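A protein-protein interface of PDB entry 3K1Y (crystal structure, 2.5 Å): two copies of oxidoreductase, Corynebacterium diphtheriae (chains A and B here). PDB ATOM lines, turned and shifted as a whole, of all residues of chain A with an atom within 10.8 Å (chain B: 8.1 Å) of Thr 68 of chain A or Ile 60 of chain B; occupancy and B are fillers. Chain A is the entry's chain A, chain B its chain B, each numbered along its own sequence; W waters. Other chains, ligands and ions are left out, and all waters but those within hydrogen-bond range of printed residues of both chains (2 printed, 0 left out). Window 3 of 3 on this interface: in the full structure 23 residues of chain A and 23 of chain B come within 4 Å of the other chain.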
ATOM      1  N   LEU A  59     -22.906  13.042 -18.591  1.00  0.00           N
ATOM      2  CA  LEU A  59     -21.712  13.839 -18.800  1.00  0.00           C
ATOM      3  C   LEU A  59     -21.378  14.678 -17.574  1.00  0.00           C
ATOM      4  O   LEU A  59     -20.515  15.554 -17.640  1.00  0.00           O
ATOM      5  CB  LEU A  59     -21.910  14.779 -19.988  1.00  0.00           C
ATOM      6  CG  LEU A  59     -22.011  14.201 -21.392  1.00  0.00           C
ATOM      7  CD1 LEU A  59     -22.043  15.366 -22.371  1.00  0.00           C
ATOM      8  CD2 LEU A  59     -20.830  13.298 -21.687  1.00  0.00           C
ATOM      9  N   ILE A  60     -22.053  14.420 -16.462  1.00  0.00           N
ATOM     10  CA  ILE A  60     -21.811  15.214 -15.267  1.00  0.00           C
ATOM     11  C   ILE A  60     -20.324  15.347 -14.913  1.00  0.00           C
ATOM     12  O   ILE A  60     -19.827  16.456 -14.729  1.00  0.00           O
ATOM     13  CB  ILE A  60     -22.613  14.662 -14.081  1.00  0.00           C
ATOM     14  CG1 ILE A  60     -24.108  14.694 -14.426  1.00  0.00           C
ATOM     15  CG2 ILE A  60     -22.361  15.513 -12.847  1.00  0.00           C
ATOM     16  CD1 ILE A  60     -25.008  14.071 -13.385  1.00  0.00           C
ATOM     17  N   PRO A  61     -19.592  14.227 -14.817  1.00  0.00           N
ATOM     18  CA  PRO A  61     -18.166  14.336 -14.488  1.00  0.00           C
ATOM     19  C   PRO A  61     -17.324  15.059 -15.545  1.00  0.00           C
ATOM     20  O   PRO A  61     -16.419  15.815 -15.201  1.00  0.00           O
ATOM     21  CB  PRO A  61     -17.735  12.883 -14.290  1.00  0.00           C
ATOM     22  CG  PRO A  61     -18.724  12.109 -15.108  1.00  0.00           C
ATOM     23  CD  PRO A  61     -20.022  12.819 -14.835  1.00  0.00           C
ATOM     24  N   ASP A  62     -17.610  14.835 -16.823  1.00  0.00           N
ATOM     25  CA  ASP A  62     -16.848  15.497 -17.883  1.00  0.00           C
ATOM     26  C   ASP A  62     -17.199  16.981 -17.914  1.00  0.00           C
ATOM     27  O   ASP A  62     -16.359  17.837 -18.215  1.00  0.00           O
ATOM     28  CB  ASP A  62     -17.169  14.883 -19.249  1.00  0.00           C
ATOM     29  CG  ASP A  62     -17.192  13.367 -19.217  1.00  0.00           C
ATOM     30  OD1 ASP A  62     -18.086  12.807 -18.544  1.00  0.00           O
ATOM     31  OD2 ASP A  62     -16.322  12.738 -19.861  1.00  0.00           O
ATOM     32  N   LEU A  63     -18.454  17.275 -17.598  1.00  0.00           N
ATOM     33  CA  LEU A  63     -18.937  18.641 -17.594  1.00  0.00           C
ATOM     34  C   LEU A  63     -18.347  19.423 -16.430  1.00  0.00           C
ATOM     35  O   LEU A  63     -17.758  20.488 -16.625  1.00  0.00           O
ATOM     36  CB  LEU A  63     -20.464  18.646 -17.516  1.00  0.00           C
ATOM     37  CG  LEU A  63     -21.227  19.405 -18.606  1.00  0.00           C
ATOM     38  CD1 LEU A  63     -20.618  19.136 -19.968  1.00  0.00           C
ATOM     39  CD2 LEU A  63     -22.683  18.977 -18.577  1.00  0.00           C
ATOM     40  N   MET A  64     -18.495  18.900 -15.221  1.00  0.00           N
ATOM     41  CA  MET A  64     -17.967  19.603 -14.073  1.00  0.00           C
ATOM     42  C   MET A  64     -16.461  19.455 -13.886  1.00  0.00           C
ATOM     43  O   MET A  64     -15.920  19.792 -12.835  1.00  0.00           O
ATOM     44  CB  MET A  64     -18.764  19.224 -12.819  1.00  0.00           C
ATOM     45  CG  MET A  64     -20.024  20.109 -12.673  1.00  0.00           C
ATOM     46  SD  MET A  64     -21.330  19.562 -11.540  1.00  0.00           S
ATOM     47  CE  MET A  64     -22.561  18.998 -12.674  1.00  0.00           C
ATOM     48  N   THR A  65     -15.789  18.943 -14.919  1.00  0.00           N
ATOM     49  CA  THR A  65     -14.329  18.839 -14.918  1.00  0.00           C
ATOM     50  C   THR A  65     -13.910  20.004 -15.802  1.00  0.00           C
ATOM     51  O   THR A  65     -12.852  20.600 -15.608  1.00  0.00           O
ATOM     52  CB  THR A  65     -13.800  17.527 -15.531  1.00  0.00           C
ATOM     53  OG1 THR A  65     -13.778  16.510 -14.527  1.00  0.00           O
ATOM     54  CG2 THR A  65     -12.375  17.705 -16.052  1.00  0.00           C
ATOM     55  N   ALA A  66     -14.762  20.324 -16.773  1.00  0.00           N
ATOM     56  CA  ALA A  66     -14.514  21.445 -17.664  1.00  0.00           C
ATOM     57  C   ALA A  66     -14.862  22.732 -16.901  1.00  0.00           C
ATOM     58  O   ALA A  66     -14.648  23.840 -17.394  1.00  0.00           O
ATOM     59  CB  ALA A  66     -15.368  21.324 -18.913  1.00  0.00           C
ATOM     60  N   MET A  67     -15.411  22.573 -15.697  1.00  0.00           N
ATOM     61  CA  MET A  67     -15.769  23.713 -14.856  1.00  0.00           C
ATOM     62  C   MET A  67     -14.579  24.087 -13.983  1.00  0.00           C
ATOM     63  O   MET A  67     -14.116  25.226 -13.989  1.00  0.00           O
ATOM     64  CB  MET A  67     -16.960  23.371 -13.953  1.00  0.00           C
ATOM     65  CG  MET A  67     -18.323  23.526 -14.607  1.00  0.00           C
ATOM     66  SD  MET A  67     -18.696  25.353 -15.129  1.00  0.00           S
ATOM     67  CE  MET A  67     -19.006  26.099 -13.373  1.00  0.00           C
ATOM     68  N   THR A  68     -14.098  23.105 -13.232  1.00  0.00           N
ATOM     69  CA  THR A  68     -12.965  23.273 -12.342  1.00  0.00           C
ATOM     70  C   THR A  68     -11.634  23.223 -13.093  1.00  0.00           C
ATOM     71  O   THR A  68     -10.571  23.132 -12.483  1.00  0.00           O
ATOM     72  CB  THR A  68     -12.991  22.191 -11.247  1.00  0.00           C
ATOM     73  OG1 THR A  68     -13.727  21.057 -11.723  1.00  0.00           O
ATOM     74  CG2 THR A  68     -13.651  22.724  -9.975  1.00  0.00           C
ATOM     75  N   THR A  69     -11.706  23.280 -14.421  1.00  0.00           N
ATOM     76  CA  THR A  69     -10.527  23.268 -15.287  1.00  0.00           C
ATOM     77  C   THR A  69     -10.993  23.660 -16.681  1.00  0.00           C
ATOM     78  O   THR A  69     -12.178  23.579 -16.979  1.00  0.00           O
ATOM     79  CB  THR A  69      -9.865  21.882 -15.359  1.00  0.00           C
ATOM     80  OG1 THR A  69      -9.421  21.484 -14.056  1.00  0.00           O
ATOM     81  CG2 THR A  69      -8.666  21.929 -16.290  1.00  0.00           C
ATOM     82  N   ARG A  70     -10.069  24.063 -17.543  1.00  0.00           N
ATOM     83  CA  ARG A  70     -10.439  24.495 -18.887  1.00  0.00           C
ATOM     84  C   ARG A  70     -10.367  23.428 -19.983  1.00  0.00           C
ATOM     85  O   ARG A  70     -10.654  23.724 -21.144  1.00  0.00           O
ATOM     86  CB  ARG A  70      -9.565  25.684 -19.299  1.00  0.00           C
ATOM     87  CG  ARG A  70      -8.113  25.299 -19.607  1.00  0.00           C
ATOM     88  CD  ARG A  70      -7.197  26.515 -19.708  1.00  0.00           C
ATOM     89  NE  ARG A  70      -5.850  26.147 -20.142  1.00  0.00           N
ATOM     90  CZ  ARG A  70      -5.086  25.229 -19.549  1.00  0.00           C
ATOM     91  NH1 ARG A  70      -5.526  24.569 -18.487  1.00  0.00           N
ATOM     92  NH2 ARG A  70      -3.874  24.967 -20.021  1.00  0.00           N
ATOM     93  N   VAL A  71      -9.993  22.197 -19.642  1.00  0.00           N
ATOM     94  CA  VAL A  71      -9.897  21.166 -20.674  1.00  0.00           C
ATOM     95  C   VAL A  71     -11.018  20.127 -20.644  1.00  0.00           C
ATOM     96  O   VAL A  71     -11.583  19.817 -19.592  1.00  0.00           O
ATOM     97  CB  VAL A  71      -8.518  20.458 -20.638  1.00  0.00           C
ATOM     98  CG1 VAL A  71      -8.448  19.378 -21.711  1.00  0.00           C
ATOM     99  CG2 VAL A  71      -7.411  21.482 -20.865  1.00  0.00           C
ATOM    100  N   HIS A  72     -11.327  19.605 -21.827  1.00  0.00           N
ATOM    101  CA  HIS A  72     -12.385  18.627 -22.008  1.00  0.00           C
ATOM    102  C   HIS A  72     -11.868  17.196 -22.088  1.00  0.00           C
ATOM    103  O   HIS A  72     -10.731  16.960 -22.483  1.00  0.00           O
ATOM    104  CB  HIS A  72     -13.164  18.946 -23.289  1.00  0.00           C
ATOM    105  CG  HIS A  72     -13.557  20.388 -23.422  1.00  0.00           C
ATOM    106  ND1 HIS A  72     -14.026  21.138 -22.364  1.00  0.00           N
ATOM    107  CD2 HIS A  72     -13.594  21.203 -24.505  1.00  0.00           C
ATOM    108  CE1 HIS A  72     -14.337  22.351 -22.787  1.00  0.00           C
ATOM    109  NE2 HIS A  72     -14.085  22.416 -24.082  1.00  0.00           N
ATOM    110  N   THR A  73     -12.706  16.241 -21.704  1.00  0.00           N
ATOM    111  CA  THR A  73     -12.330  14.831 -21.773  1.00  0.00           C
ATOM    112  C   THR A  73     -12.409  14.417 -23.240  1.00  0.00           C
ATOM    113  O   THR A  73     -13.008  15.122 -24.050  1.00  0.00           O
ATOM    114  CB  THR A  73     -13.317  13.926 -21.002  1.00  0.00           C
ATOM    115  OG1 THR A  73     -14.643  14.130 -21.509  1.00  0.00           O
ATOM    116  CG2 THR A  73     -13.283  14.221 -19.523  1.00  0.00           C
ATOM    117  N   LEU A  76     -16.010  14.498 -24.225  1.00  0.00           N
ATOM    118  CA  LEU A  76     -16.593  15.818 -24.446  1.00  0.00           C
ATOM    119  C   LEU A  76     -16.055  16.453 -25.729  1.00  0.00           C
ATOM    120  O   LEU A  76     -16.805  17.107 -26.462  1.00  0.00           O
ATOM    121  CB  LEU A  76     -16.313  16.716 -23.238  1.00  0.00           C
ATOM    122  CG  LEU A  76     -16.990  18.086 -23.104  1.00  0.00           C
ATOM    123  CD1 LEU A  76     -18.482  18.001 -23.419  1.00  0.00           C
ATOM    124  CD2 LEU A  76     -16.775  18.585 -21.680  1.00  0.00           C
ATOM    125  N   LEU A 103     -27.881  22.413 -15.349  1.00  0.00           N
ATOM    126  CA  LEU A 103     -27.039  21.456 -16.062  1.00  0.00           C
ATOM    127  C   LEU A 103     -27.120  21.692 -17.574  1.00  0.00           C
ATOM    128  O   LEU A 103     -26.120  21.598 -18.291  1.00  0.00           O
ATOM    129  CB  LEU A 103     -27.460  20.024 -15.730  1.00  0.00           C
ATOM    130  CG  LEU A 103     -26.699  18.896 -16.445  1.00  0.00           C
ATOM    131  CD1 LEU A 103     -25.245  18.880 -15.986  1.00  0.00           C
ATOM    132  CD2 LEU A 103     -27.379  17.549 -16.150  1.00  0.00           C
ATOM    133  N   MET A 106     -25.127  24.711 -18.143  1.00  0.00           N
ATOM    134  CA  MET A 106     -23.709  24.449 -18.015  1.00  0.00           C
ATOM    135  C   MET A 106     -23.100  23.992 -19.329  1.00  0.00           C
ATOM    136  O   MET A 106     -22.070  24.510 -19.756  1.00  0.00           O
ATOM    137  CB  MET A 106     -23.473  23.400 -16.940  1.00  0.00           C
ATOM    138  CG  MET A 106     -22.025  23.267 -16.526  1.00  0.00           C
ATOM    139  SD  MET A 106     -21.895  22.119 -14.996  1.00  0.00           S
ATOM    140  CE  MET A 106     -22.474  23.378 -13.630  1.00  0.00           C
ATOM    141  N   ILE A 110     -20.045  25.824 -21.563  1.00  0.00           N
ATOM    142  CA  ILE A 110     -18.796  25.152 -21.905  1.00  0.00           C
ATOM    143  C   ILE A 110     -18.371  25.237 -23.371  1.00  0.00           C
ATOM    144  O   ILE A 110     -17.197  25.065 -23.686  1.00  0.00           O
ATOM    145  CB  ILE A 110     -18.870  23.649 -21.459  1.00  0.00           C
ATOM    146  CG1 ILE A 110     -17.732  23.349 -20.497  1.00  0.00           C
ATOM    147  CG2 ILE A 110     -18.817  22.701 -22.654  1.00  0.00           C
ATOM    148  CD1 ILE A 110     -17.811  24.128 -19.200  1.00  0.00           C
ATOM    149  N   ALA B  19     -21.075  33.391  -7.518  1.00  0.00           N
ATOM    150  CA  ALA B  19     -20.865  32.239  -8.396  1.00  0.00           C
ATOM    151  C   ALA B  19     -19.711  32.346  -9.377  1.00  0.00           C
ATOM    152  O   ALA B  19     -19.658  31.597 -10.348  1.00  0.00           O
ATOM    153  CB  ALA B  19     -22.161  31.928  -9.154  1.00  0.00           C
ATOM    154  N   GLY B  20     -18.782  33.260  -9.128  1.00  0.00           N
ATOM    155  CA  GLY B  20     -17.651  33.405 -10.031  1.00  0.00           C
ATOM    156  C   GLY B  20     -16.673  32.239  -9.998  1.00  0.00           C
ATOM    157  O   GLY B  20     -16.642  31.466  -9.036  1.00  0.00           O
ATOM    158  N   LEU B  21     -15.872  32.109 -11.055  1.00  0.00           N
ATOM    159  CA  LEU B  21     -14.869  31.043 -11.147  1.00  0.00           C
ATOM    160  C   LEU B  21     -13.443  31.591 -11.235  1.00  0.00           C
ATOM    161  O   LEU B  21     -12.497  30.833 -11.448  1.00  0.00           O
ATOM    162  CB  LEU B  21     -15.138  30.151 -12.365  1.00  0.00           C
ATOM    163  CG  LEU B  21     -16.248  29.101 -12.258  1.00  0.00           C
ATOM    164  CD1 LEU B  21     -17.574  29.790 -12.042  1.00  0.00           C
ATOM    165  CD2 LEU B  21     -16.298  28.258 -13.521  1.00  0.00           C
ATOM    166  N   GLU B  55     -19.376  30.536  -1.696  1.00  0.00           N
ATOM    167  CA  GLU B  55     -18.769  30.568  -3.028  1.00  0.00           C
ATOM    168  C   GLU B  55     -19.149  29.279  -3.765  1.00  0.00           C
ATOM    169  O   GLU B  55     -18.669  28.201  -3.425  1.00  0.00           O
ATOM    170  CB  GLU B  55     -17.240  30.667  -2.925  1.00  0.00           C
ATOM    171  CG  GLU B  55     -16.682  32.039  -2.575  1.00  0.00           C
ATOM    172  CD  GLU B  55     -16.500  32.930  -3.797  1.00  0.00           C
ATOM    173  OE1 GLU B  55     -16.706  32.436  -4.932  1.00  0.00           O
ATOM    174  OE2 GLU B  55     -16.142  34.122  -3.627  1.00  0.00           O
ATOM    175  N   LEU B  56     -20.006  29.387  -4.778  1.00  0.00           N
ATOM    176  CA  LEU B  56     -20.438  28.212  -5.533  1.00  0.00           C
ATOM    177  C   LEU B  56     -19.303  27.414  -6.145  1.00  0.00           C
ATOM    178  O   LEU B  56     -19.382  26.197  -6.235  1.00  0.00           O
ATOM    179  CB  LEU B  56     -21.426  28.610  -6.630  1.00  0.00           C
ATOM    180  CG  LEU B  56     -22.798  29.094  -6.152  1.00  0.00           C
ATOM    181  CD1 LEU B  56     -23.747  29.198  -7.354  1.00  0.00           C
ATOM    182  CD2 LEU B  56     -23.355  28.131  -5.108  1.00  0.00           C
ATOM    183  N   SER B  57     -18.240  28.088  -6.558  1.00  0.00           N
ATOM    184  CA  SER B  57     -17.101  27.394  -7.148  1.00  0.00           C
ATOM    185  C   SER B  57     -16.514  26.387  -6.152  1.00  0.00           C
ATOM    186  O   SER B  57     -15.802  25.462  -6.530  1.00  0.00           O
ATOM    187  CB  SER B  57     -16.033  28.402  -7.557  1.00  0.00           C
ATOM    188  OG  SER B  57     -15.606  29.160  -6.435  1.00  0.00           O
ATOM    189  N   GLU B  58     -16.830  26.566  -4.878  1.00  0.00           N
ATOM    190  CA  GLU B  58     -16.331  25.679  -3.840  1.00  0.00           C
ATOM    191  C   GLU B  58     -17.308  24.555  -3.491  1.00  0.00           C
ATOM    192  O   GLU B  58     -17.060  23.787  -2.563  1.00  0.00           O
ATOM    193  CB  GLU B  58     -16.002  26.490  -2.580  1.00  0.00           C
ATOM    194  CG  GLU B  58     -14.683  27.252  -2.658  1.00  0.00           C
ATOM    195  CD  GLU B  58     -14.588  28.375  -1.634  1.00  0.00           C
ATOM    196  OE1 GLU B  58     -15.297  28.299  -0.604  1.00  0.00           O
ATOM    197  OE2 GLU B  58     -13.797  29.327  -1.855  1.00  0.00           O
ATOM    198  N   LEU B  59     -18.414  24.457  -4.225  1.00  0.00           N
ATOM    199  CA  LEU B  59     -19.402  23.414  -3.959  1.00  0.00           C
ATOM    200  C   LEU B  59     -19.689  22.556  -5.187  1.00  0.00           C
ATOM    201  O   LEU B  59     -20.634  21.757  -5.195  1.00  0.00           O
ATOM    202  CB  LEU B  59     -20.708  24.036  -3.467  1.00  0.00           C
ATOM    203  CG  LEU B  59     -20.652  24.837  -2.170  1.00  0.00           C
ATOM    204  CD1 LEU B  59     -22.063  25.269  -1.803  1.00  0.00           C
ATOM    205  CD2 LEU B  59     -20.056  23.996  -1.071  1.00  0.00           C
ATOM    206  N   ILE B  60     -18.870  22.728  -6.220  1.00  0.00           N
ATOM    207  CA  ILE B  60     -19.026  21.984  -7.463  1.00  0.00           C
ATOM    208  C   ILE B  60     -19.139  20.473  -7.250  1.00  0.00           C
ATOM    209  O   ILE B  60     -19.959  19.814  -7.887  1.00  0.00           O
ATOM    210  CB  ILE B  60     -17.871  22.314  -8.425  1.00  0.00           C
ATOM    211  CG1 ILE B  60     -17.988  23.782  -8.854  1.00  0.00           C
ATOM    212  CG2 ILE B  60     -17.910  21.406  -9.639  1.00  0.00           C
ATOM    213  CD1 ILE B  60     -16.843  24.277  -9.715  1.00  0.00           C
ATOM    214  N   PRO B  61     -18.321  19.903  -6.349  1.00  0.00           N
ATOM    215  CA  PRO B  61     -18.399  18.457  -6.108  1.00  0.00           C
ATOM    216  C   PRO B  61     -19.742  18.053  -5.495  1.00  0.00           C
ATOM    217  O   PRO B  61     -20.379  17.103  -5.949  1.00  0.00           O
ATOM    218  CB  PRO B  61     -17.238  18.200  -5.146  1.00  0.00           C
ATOM    219  CG  PRO B  61     -16.257  19.274  -5.504  1.00  0.00           C
ATOM    220  CD  PRO B  61     -17.149  20.481  -5.671  1.00  0.00           C
ATOM    221  N   ASP B  62     -20.165  18.779  -4.462  1.00  0.00           N
ATOM    222  CA  ASP B  62     -21.428  18.499  -3.777  1.00  0.00           C
ATOM    223  C   ASP B  62     -22.608  18.707  -4.725  1.00  0.00           C
ATOM    224  O   ASP B  62     -23.564  17.928  -4.730  1.00  0.00           O
ATOM    225  CB  ASP B  62     -21.590  19.423  -2.562  1.00  0.00           C
ATOM    226  CG  ASP B  62     -20.345  19.474  -1.696  1.00  0.00           C
ATOM    227  OD1 ASP B  62     -19.310  19.994  -2.181  1.00  0.00           O
ATOM    228  OD2 ASP B  62     -20.403  18.994  -0.535  1.00  0.00           O
ATOM    229  N   LEU B  63     -22.534  19.779  -5.506  1.00  0.00           N
ATOM    230  CA  LEU B  63     -23.572  20.109  -6.473  1.00  0.00           C
ATOM    231  C   LEU B  63     -23.674  18.981  -7.495  1.00  0.00           C
ATOM    232  O   LEU B  63     -24.772  18.571  -7.877  1.00  0.00           O
ATOM    233  CB  LEU B  63     -23.227  21.426  -7.173  1.00  0.00           C
ATOM    234  CG  LEU B  63     -24.006  22.697  -6.819  1.00  0.00           C
ATOM    235  CD1 LEU B  63     -24.845  22.511  -5.569  1.00  0.00           C
ATOM    236  CD2 LEU B  63     -23.017  23.839  -6.651  1.00  0.00           C
ATOM    237  N   MET B  64     -22.517  18.483  -7.922  1.00  0.00           N
ATOM    238  CA  MET B  64     -22.447  17.394  -8.885  1.00  0.00           C
ATOM    239  C   MET B  64     -23.149  16.171  -8.312  1.00  0.00           C
ATOM    240  O   MET B  64     -23.936  15.515  -8.989  1.00  0.00           O
ATOM    241  CB  MET B  64     -20.981  17.052  -9.182  1.00  0.00           C
ATOM    242  CG  MET B  64     -20.782  15.963 -10.234  1.00  0.00           C
ATOM    243  SD  MET B  64     -19.785  14.388  -9.660  1.00  0.00           S
ATOM    244  CE  MET B  64     -21.252  13.215  -9.212  1.00  0.00           C
ATOM    245  N   THR B  65     -22.860  15.876  -7.049  1.00  0.00           N
ATOM    246  CA  THR B  65     -23.447  14.724  -6.378  1.00  0.00           C
ATOM    247  C   THR B  65     -24.958  14.830  -6.316  1.00  0.00           C
ATOM    248  O   THR B  65     -25.668  13.849  -6.546  1.00  0.00           O
ATOM    249  CB  THR B  65     -22.901  14.560  -4.943  1.00  0.00           C
ATOM    250  OG1 THR B  65     -21.486  14.339  -4.989  1.00  0.00           O
ATOM    251  CG2 THR B  65     -23.563  13.375  -4.254  1.00  0.00           C
ATOM    252  N   ALA B  66     -25.452  16.023  -6.011  1.00  0.00           N
ATOM    253  CA  ALA B  66     -26.888  16.228  -5.928  1.00  0.00           C
ATOM    254  C   ALA B  66     -27.579  16.066  -7.286  1.00  0.00           C
ATOM    255  O   ALA B  66     -28.805  16.070  -7.360  1.00  0.00           O
ATOM    256  CB  ALA B  66     -27.183  17.598  -5.349  1.00  0.00           C
ATOM    257  N   MET B  67     -26.803  15.927  -8.358  1.00  0.00           N
ATOM    258  CA  MET B  67     -27.391  15.760  -9.683  1.00  0.00           C
ATOM    259  C   MET B  67     -27.516  14.286 -10.052  1.00  0.00           C
ATOM    260  O   MET B  67     -28.526  13.862 -10.604  1.00  0.00           O
ATOM    261  CB  MET B  67     -26.559  16.487 -10.742  1.00  0.00           C
ATOM    262  CG  MET B  67     -26.597  18.017 -10.662  1.00  0.00           C
ATOM    263  SD  MET B  67     -28.327  18.821 -11.049  1.00  0.00           S
ATOM    264  CE  MET B  67     -28.307  18.676 -12.972  1.00  0.00           C
ATOM    265  N   LYS B  75     -22.204  18.712   3.880  1.00  0.00           N
ATOM    266  CA  LYS B  75     -21.741  20.060   3.594  1.00  0.00           C
ATOM    267  C   LYS B  75     -22.837  20.900   2.940  1.00  0.00           C
ATOM    268  O   LYS B  75     -23.197  21.969   3.435  1.00  0.00           O
ATOM    269  CB  LYS B  75     -20.518  20.009   2.681  1.00  0.00           C
ATOM    270  CG  LYS B  75     -19.914  21.357   2.376  1.00  0.00           C
ATOM    271  CD  LYS B  75     -18.718  21.212   1.453  1.00  0.00           C
ATOM    272  CE  LYS B  75     -17.965  22.526   1.316  1.00  0.00           C
ATOM    273  NZ  LYS B  75     -16.725  22.350   0.506  1.00  0.00           N
ATOM    274  N   LEU B 103     -23.845  26.939 -13.324  1.00  0.00           N
ATOM    275  CA  LEU B 103     -23.559  26.570 -11.947  1.00  0.00           C
ATOM    276  C   LEU B 103     -24.496  27.355 -11.023  1.00  0.00           C
ATOM    277  O   LEU B 103     -25.060  26.802 -10.077  1.00  0.00           O
ATOM    278  CB  LEU B 103     -22.096  26.877 -11.620  1.00  0.00           C
ATOM    279  CG  LEU B 103     -21.662  26.647 -10.168  1.00  0.00           C
ATOM    280  CD1 LEU B 103     -21.799  25.174  -9.807  1.00  0.00           C
ATOM    281  CD2 LEU B 103     -20.233  27.115  -9.987  1.00  0.00           C
ATOM    282  N   MET B 106     -27.834  25.913 -10.967  1.00  0.00           N
ATOM    283  CA  MET B 106     -27.795  24.576 -10.380  1.00  0.00           C
ATOM    284  C   MET B 106     -27.997  24.573  -8.866  1.00  0.00           C
ATOM    285  O   MET B 106     -28.655  23.691  -8.324  1.00  0.00           O
ATOM    286  CB  MET B 106     -26.471  23.891 -10.719  1.00  0.00           C
ATOM    287  CG  MET B 106     -26.498  22.400 -10.471  1.00  0.00           C
ATOM    288  SD  MET B 106     -25.002  21.475 -11.253  1.00  0.00           S
ATOM    289  CE  MET B 106     -25.358  21.824 -13.119  1.00  0.00           C
ATOM    290  N   ILE B 110     -31.491  22.818  -6.927  1.00  0.00           N
ATOM    291  CA  ILE B 110     -31.384  21.864  -5.846  1.00  0.00           C
ATOM    292  C   ILE B 110     -32.093  22.290  -4.567  1.00  0.00           C
ATOM    293  O   ILE B 110     -32.378  21.456  -3.706  1.00  0.00           O
ATOM    294  CB  ILE B 110     -29.895  21.597  -5.574  1.00  0.00           C
ATOM    295  CG1 ILE B 110     -29.331  20.751  -6.716  1.00  0.00           C
ATOM    296  CG2 ILE B 110     -29.700  20.922  -4.235  1.00  0.00           C
ATOM    297  CD1 ILE B 110     -27.826  20.610  -6.697  1.00  0.00           C
HETATM  298  O   HOH W   1     -21.742  27.116 -15.189  1.00  0.00           O
HETATM  299  O   HOH W   2     -29.435  22.030 -12.593  1.00  0.00           O
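Water W1 lies within hydrogen-bond range of N of Leu 103 of chain B and SD of Met 67 of chain A.
Water W2 lies within hydrogen-bond range of the backbone NH of Leu 103 of chain A (3.2 Å) and the side-chain sulfur of Met 67 of chain B (3.7 Å).
Asp 62 of chain A touches none of the printed residues of chain B.
Of the printed residues of chain B, Met 64 of chain A touches Ile 60 (3.9 Å), Met 64 (3.5 Å) and Met 106 (3.8 Å).
Of chain B, only Ile 60 comes within 4 Å of Thr 68 of chain A.
No residue of chain A comes within 4 Å of Ser 57 of chain B.
No residue of chain A comes within 4 Å of Leu 59 of chain B.
Ile 60 of chain B touches just these residues of chain A: Met 64 (3.9 Å) and Thr 68 (3.6 Å).
No residue of chain A comes within 4 Å of Leu 63 of chain B.
Of the printed residues of chain A, Met 106 of chain B touches Met 64, Leu 103 and Met 106.
The nearest residue of chain B that does not touch Thr 68 of chain A is Ser 57 of chain B (4.9 Å).
The nearest residue of chain A that does not touch Ile 60 of chain B is Met 67 of chain A (4.3 Å).
Among the printed residues, merely in contact across the chains: Ile 60 of chain A with Met 64 of chain B, Leu 103 of chain A with Met 67 of chain B, Met 106 of chain A with Met 106 of chain B, Leu 103 of chain A with Met 106 of chain B, Met 64 of chain A with Met 64 of chain B, Met 67 of chain A with Leu 21 of chain B, Thr 68 of chain A with Ile 60 of chain B, Met 67 of chain A with Leu 103 of chain B, Met 64 of chain A with Met 106 of chain B, Met 106 of chain A with Leu 103 of chain B, Ile 60 of chain A with Met 67 of chain B and Met 64 of chain A with Ile 60 of chain B.
Of the 20 printed residues of chain B, 6 touch a printed residue of chain A.
Hydrophobic or aromatic side chains of chain B that line the printed part of chain A: Leu 21, Ile 60, Met 64, Met 67, Leu 103 and Met 106.
Hydrophobic or aromatic side chains of chain A that line the printed part of chain B: Ile 60, Met 64, Met 67, Leu 103 and Met 106.
Among the printed residues, 12 pairs touch across the chains.
Among the printed residues, no Asp or Glu carboxylate lies within 4 Å of a Lys or Arg side-chain nitrogen of the other chain.
Ile 60 of chain A touches Met 64 of chain B, and with the chains exchanged Met 64 of chain A touches Ile 60 of chain B.
Ile 60 of chain A touches Met 67 of chain B, but with the chains exchanged Met 67 of chain A does not touch Ile 60 of chain B (4.3 Å).
Met 64 of chain B touches its own counterpart, Met 64 of chain A.
Met 106 of chain A touches its own counterpart, Met 106 of chain B.
The backbone carbonyl oxygen (O) of Met 64 of chain A is in hydrogen-bond range of the side-chain hydroxyl (OG1) of Thr 68 of chain A (2.8 Å).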
